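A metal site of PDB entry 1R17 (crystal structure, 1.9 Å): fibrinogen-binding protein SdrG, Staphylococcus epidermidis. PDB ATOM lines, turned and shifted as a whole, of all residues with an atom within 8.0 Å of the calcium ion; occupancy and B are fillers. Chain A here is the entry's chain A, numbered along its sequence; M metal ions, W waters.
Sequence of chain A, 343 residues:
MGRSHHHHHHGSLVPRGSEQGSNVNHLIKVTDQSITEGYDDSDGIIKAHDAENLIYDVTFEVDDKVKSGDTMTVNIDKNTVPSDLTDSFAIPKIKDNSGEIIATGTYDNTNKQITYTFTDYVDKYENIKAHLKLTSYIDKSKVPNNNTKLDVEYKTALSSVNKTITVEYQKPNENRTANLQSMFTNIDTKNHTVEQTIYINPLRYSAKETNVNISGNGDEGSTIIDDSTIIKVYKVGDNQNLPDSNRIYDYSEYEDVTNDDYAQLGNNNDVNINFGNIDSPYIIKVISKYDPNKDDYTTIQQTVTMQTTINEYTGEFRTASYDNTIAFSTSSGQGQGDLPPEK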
ATOM      1  N   THR A  36      14.378 -12.885  11.318  1.00  0.00           N
ATOM      2  CA  THR A  36      14.711 -14.272  11.010  1.00  0.00           C
ATOM      3  C   THR A  36      13.501 -15.183  10.971  1.00  0.00           C
ATOM      4  O   THR A  36      12.607 -15.068  11.803  1.00  0.00           O
ATOM      5  CB  THR A  36      15.694 -14.817  12.063  1.00  0.00           C
ATOM      6  OG1 THR A  36      16.794 -13.921  12.202  1.00  0.00           O
ATOM      7  CG2 THR A  36      16.205 -16.190  11.657  1.00  0.00           C
ATOM      8  N   GLU A  37      13.482 -16.093  10.012  1.00  0.00           N
ATOM      9  CA  GLU A  37      12.391 -17.048   9.890  1.00  0.00           C
ATOM     10  C   GLU A  37      12.594 -18.151  10.919  1.00  0.00           C
ATOM     11  O   GLU A  37      13.715 -18.598  11.137  1.00  0.00           O
ATOM     12  CB  GLU A  37      12.379 -17.643   8.478  1.00  0.00           C
ATOM     13  CG  GLU A  37      12.228 -16.590   7.386  1.00  0.00           C
ATOM     14  CD  GLU A  37      12.237 -17.202   6.005  1.00  0.00           C
ATOM     15  OE1 GLU A  37      11.421 -18.118   5.761  1.00  0.00           O
ATOM     16  OE2 GLU A  37      13.072 -16.781   5.176  1.00  0.00           O
ATOM     17  N   GLY A  38      11.507 -18.587  11.551  1.00  0.00           N
ATOM     18  CA  GLY A  38      11.591 -19.610  12.585  1.00  0.00           C
ATOM     19  C   GLY A  38      12.199 -20.942  12.170  1.00  0.00           C
ATOM     20  O   GLY A  38      12.855 -21.610  12.977  1.00  0.00           O
ATOM     21  N   TYR A  39      11.978 -21.339  10.924  1.00  0.00           N
ATOM     22  CA  TYR A  39      12.521 -22.605  10.431  1.00  0.00           C
ATOM     23  C   TYR A  39      13.663 -22.325   9.456  1.00  0.00           C
ATOM     24  O   TYR A  39      13.801 -21.198   8.961  1.00  0.00           O
ATOM     25  CB  TYR A  39      11.396 -23.408   9.761  1.00  0.00           C
ATOM     26  CG  TYR A  39      10.240 -23.698  10.694  1.00  0.00           C
ATOM     27  CD1 TYR A  39       8.942 -23.858  10.213  1.00  0.00           C
ATOM     28  CD2 TYR A  39      10.445 -23.820  12.076  1.00  0.00           C
ATOM     29  CE1 TYR A  39       7.871 -24.128  11.074  1.00  0.00           C
ATOM     30  CE2 TYR A  39       9.387 -24.088  12.942  1.00  0.00           C
ATOM     31  CZ  TYR A  39       8.108 -24.242  12.428  1.00  0.00           C
ATOM     32  OH  TYR A  39       7.054 -24.521  13.285  1.00  0.00           O
ATOM     33  N   ASP A  40      14.478 -23.335   9.184  1.00  0.00           N
ATOM     34  CA  ASP A  40      15.627 -23.149   8.289  1.00  0.00           C
ATOM     35  C   ASP A  40      15.518 -23.853   6.933  1.00  0.00           C
ATOM     36  O   ASP A  40      16.417 -23.720   6.098  1.00  0.00           O
ATOM     37  CB  ASP A  40      16.908 -23.637   8.978  1.00  0.00           C
ATOM     38  CG  ASP A  40      17.398 -22.662  10.038  1.00  0.00           C
ATOM     39  OD1 ASP A  40      18.264 -23.060  10.854  1.00  0.00           O
ATOM     40  OD2 ASP A  40      16.931 -21.497  10.064  1.00  0.00           O
ATOM     41  N   ASP A  41      14.432 -24.587   6.713  1.00  0.00           N
ATOM     42  CA  ASP A  41      14.278 -25.313   5.452  1.00  0.00           C
ATOM     43  C   ASP A  41      13.284 -24.721   4.453  1.00  0.00           C
ATOM     44  O   ASP A  41      12.824 -25.415   3.540  1.00  0.00           O
ATOM     45  CB  ASP A  41      13.910 -26.769   5.764  1.00  0.00           C
ATOM     46  CG  ASP A  41      12.631 -26.898   6.556  1.00  0.00           C
ATOM     47  OD1 ASP A  41      12.235 -25.929   7.237  1.00  0.00           O
ATOM     48  OD2 ASP A  41      12.008 -27.998   6.518  1.00  0.00           O
ATOM     49  N   SER A  42      12.969 -23.435   4.601  1.00  0.00           N
ATOM     50  CA  SER A  42      12.041 -22.769   3.688  1.00  0.00           C
ATOM     51  C   SER A  42      12.335 -21.278   3.586  1.00  0.00           C
ATOM     52  O   SER A  42      11.425 -20.448   3.708  1.00  0.00           O
ATOM     53  CB  SER A  42      10.592 -23.003   4.133  1.00  0.00           C
ATOM     54  OG  SER A  42      10.383 -22.604   5.476  1.00  0.00           O
ATOM     55  N   ASP A  43      13.599 -20.941   3.362  1.00  0.00           N
ATOM     56  CA  ASP A  43      14.028 -19.544   3.258  1.00  0.00           C
ATOM     57  C   ASP A  43      13.177 -18.737   2.287  1.00  0.00           C
ATOM     58  O   ASP A  43      12.847 -19.194   1.195  1.00  0.00           O
ATOM     59  CB  ASP A  43      15.495 -19.467   2.824  1.00  0.00           C
ATOM     60  CG  ASP A  43      16.397 -20.358   3.644  1.00  0.00           C
ATOM     61  OD1 ASP A  43      16.249 -21.604   3.565  1.00  0.00           O
ATOM     62  OD2 ASP A  43      17.263 -19.822   4.378  1.00  0.00           O
ATOM     63  N   GLY A  44      12.821 -17.515   2.699  1.00  0.00           N
ATOM     64  CA  GLY A  44      12.023 -16.650   1.850  1.00  0.00           C
ATOM     65  C   GLY A  44      10.529 -16.908   1.928  1.00  0.00           C
ATOM     66  O   GLY A  44       9.722 -16.127   1.430  1.00  0.00           O
ATOM     67  N   ILE A  45      10.157 -18.022   2.561  1.00  0.00           N
ATOM     68  CA  ILE A  45       8.754 -18.399   2.701  1.00  0.00           C
ATOM     69  C   ILE A  45       8.357 -18.634   4.156  1.00  0.00           C
ATOM     70  O   ILE A  45       9.055 -19.348   4.887  1.00  0.00           O
ATOM     71  CB  ILE A  45       8.441 -19.703   1.930  1.00  0.00           C
ATOM     72  CG1 ILE A  45       8.741 -19.534   0.433  1.00  0.00           C
ATOM     73  CG2 ILE A  45       6.966 -20.091   2.127  1.00  0.00           C
ATOM     74  CD1 ILE A  45       8.527 -20.801  -0.377  1.00  0.00           C
ATOM     75  N   ILE A  46       7.251 -18.045   4.578  1.00  0.00           N
ATOM     76  CA  ILE A  46       6.779 -18.249   5.933  1.00  0.00           C
ATOM     77  C   ILE A  46       5.633 -19.246   5.856  1.00  0.00           C
ATOM     78  O   ILE A  46       4.576 -18.960   5.293  1.00  0.00           O
ATOM     79  CB  ILE A  46       6.268 -16.945   6.595  1.00  0.00           C
ATOM     80  CG1 ILE A  46       7.438 -15.985   6.810  1.00  0.00           C
ATOM     81  CG2 ILE A  46       5.597 -17.268   7.917  1.00  0.00           C
ATOM     82  CD1 ILE A  46       8.545 -16.548   7.695  1.00  0.00           C
ATOM     83  N   LYS A  47       5.868 -20.438   6.391  1.00  0.00           N
ATOM     84  CA  LYS A  47       4.868 -21.493   6.391  1.00  0.00           C
ATOM     85  C   LYS A  47       3.976 -21.256   7.589  1.00  0.00           C
ATOM     86  O   LYS A  47       4.114 -21.906   8.625  1.00  0.00           O
ATOM     87  CB  LYS A  47       5.575 -22.845   6.482  1.00  0.00           C
ATOM     88  CG  LYS A  47       6.618 -23.078   5.392  1.00  0.00           C
ATOM     89  CD  LYS A  47       6.003 -23.627   4.118  1.00  0.00           C
ATOM     90  CE  LYS A  47       7.070 -23.948   3.077  1.00  0.00           C
ATOM     91  NZ  LYS A  47       6.490 -24.720   1.937  1.00  0.00           N
ATOM     92  N   ALA A  48       3.078 -20.286   7.457  1.00  0.00           N
ATOM     93  CA  ALA A  48       2.163 -19.925   8.544  1.00  0.00           C
ATOM     94  C   ALA A  48       1.399 -21.116   9.097  1.00  0.00           C
ATOM     95  O   ALA A  48       1.162 -21.186  10.299  1.00  0.00           O
ATOM     96  CB  ALA A  48       1.181 -18.858   8.065  1.00  0.00           C
ATOM     97  N   GLU A  52       5.280 -21.421  11.498  1.00  0.00           N
ATOM     98  CA  GLU A  52       6.581 -20.754  11.399  1.00  0.00           C
ATOM     99  C   GLU A  52       6.463 -19.299  11.821  1.00  0.00           C
ATOM    100  O   GLU A  52       5.639 -18.558  11.281  1.00  0.00           O
ATOM    101  CB  GLU A  52       7.150 -20.832   9.968  1.00  0.00           C
ATOM    102  CG  GLU A  52       8.625 -20.408   9.903  1.00  0.00           C
ATOM    103  CD  GLU A  52       9.246 -20.534   8.509  1.00  0.00           C
ATOM    104  OE1 GLU A  52      10.493 -20.410   8.415  1.00  0.00           O
ATOM    105  OE2 GLU A  52       8.511 -20.727   7.515  1.00  0.00           O
ATOM    106  N   ASN A  53       7.290 -18.893  12.772  1.00  0.00           N
ATOM    107  CA  ASN A  53       7.274 -17.522  13.278  1.00  0.00           C
ATOM    108  C   ASN A  53       8.316 -16.605  12.629  1.00  0.00           C
ATOM    109  O   ASN A  53       9.207 -17.065  11.917  1.00  0.00           O
ATOM    110  CB  ASN A  53       7.460 -17.535  14.799  1.00  0.00           C
ATOM    111  CG  ASN A  53       8.732 -18.263  15.247  1.00  0.00           C
ATOM    112  OD1 ASN A  53       9.138 -19.250  14.650  1.00  0.00           O
ATOM    113  ND2 ASN A  53       9.344 -17.774  16.323  1.00  0.00           N
ATOM    114  N   LEU A  54       8.161 -15.305  12.855  1.00  0.00           N
ATOM    115  CA  LEU A  54       9.102 -14.295  12.367  1.00  0.00           C
ATOM    116  C   LEU A  54       9.769 -13.747  13.623  1.00  0.00           C
ATOM    117  O   LEU A  54       9.094 -13.218  14.507  1.00  0.00           O
ATOM    118  CB  LEU A  54       8.362 -13.172  11.636  1.00  0.00           C
ATOM    119  CG  LEU A  54       8.023 -13.459  10.173  1.00  0.00           C
ATOM    120  CD1 LEU A  54       7.082 -12.391   9.621  1.00  0.00           C
ATOM    121  CD2 LEU A  54       9.304 -13.505   9.357  1.00  0.00           C
ATOM    122  N   LYS A 163      12.444  -7.046   5.233  1.00  0.00           N
ATOM    123  CA  LYS A 163      12.748  -8.372   4.710  1.00  0.00           C
ATOM    124  C   LYS A 163      11.575  -8.839   3.858  1.00  0.00           C
ATOM    125  O   LYS A 163      10.425  -8.769   4.283  1.00  0.00           O
ATOM    126  CB  LYS A 163      12.977  -9.374   5.841  1.00  0.00           C
ATOM    127  CG  LYS A 163      13.405 -10.749   5.371  1.00  0.00           C
ATOM    128  CD  LYS A 163      13.566 -11.718   6.531  1.00  0.00           C
ATOM    129  CE  LYS A 163      14.706 -12.706   6.313  1.00  0.00           C
ATOM    130  NZ  LYS A 163      14.476 -13.618   5.164  1.00  0.00           N
ATOM    131  N   ILE A 165       9.320 -11.621   2.163  1.00  0.00           N
ATOM    132  CA  ILE A 165       8.950 -13.011   2.371  1.00  0.00           C
ATOM    133  C   ILE A 165       7.598 -13.284   1.729  1.00  0.00           C
ATOM    134  O   ILE A 165       6.823 -12.360   1.484  1.00  0.00           O
ATOM    135  CB  ILE A 165       8.833 -13.367   3.875  1.00  0.00           C
ATOM    136  CG1 ILE A 165       7.905 -12.359   4.565  1.00  0.00           C
ATOM    137  CG2 ILE A 165      10.217 -13.382   4.518  1.00  0.00           C
ATOM    138  CD1 ILE A 165       7.628 -12.667   6.007  1.00  0.00           C
ATOM    139  N   THR A 166       7.330 -14.545   1.441  1.00  0.00           N
ATOM    140  CA  THR A 166       6.063 -14.927   0.856  1.00  0.00           C
ATOM    141  C   THR A 166       5.345 -15.802   1.871  1.00  0.00           C
ATOM    142  O   THR A 166       5.937 -16.714   2.446  1.00  0.00           O
ATOM    143  CB  THR A 166       6.267 -15.705  -0.455  1.00  0.00           C
ATOM    144  OG1 THR A 166       6.929 -14.856  -1.410  1.00  0.00           O
ATOM    145  CG2 THR A 166       4.934 -16.164  -1.017  1.00  0.00           C
HETATM  146 CA    CA M   1      10.619 -20.333   6.052  1.00  0.00          CA
HETATM  147  O   HOH W   1      12.958 -20.841   6.510  1.00  0.00           O
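The side-chain carboxylate (OE1) of Glu 52 sits close to the backbone NH (N) of Tyr 39, 3.1 Å away. O of Lys 47 lies within hydrogen-bond range of N of Glu 52. N of Gly 44 lies within hydrogen-bond range of OE2 of Glu 37, 2.6 Å away. OE2 of Glu 37 lies within salt-bridge range of NZ of Lys 163 (3.5 Å).
O of Ile 45 binds the calcium ion, at 2.2 Å. The calcium ion is bound by OG of Ser 42, 2.4 Å away. The side-chain carboxylate (OE1) of Glu 52 binds the calcium ion, 2.4 Å away. OE1 of Glu 37 binds the calcium ion. Water W1 is bound to the calcium ion, 2.4 Å away. The backbone carbonyl oxygen (O) of Ser 42 binds the calcium ion (2.5 Å). The calcium ion is bound by OE2 of Glu 52.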
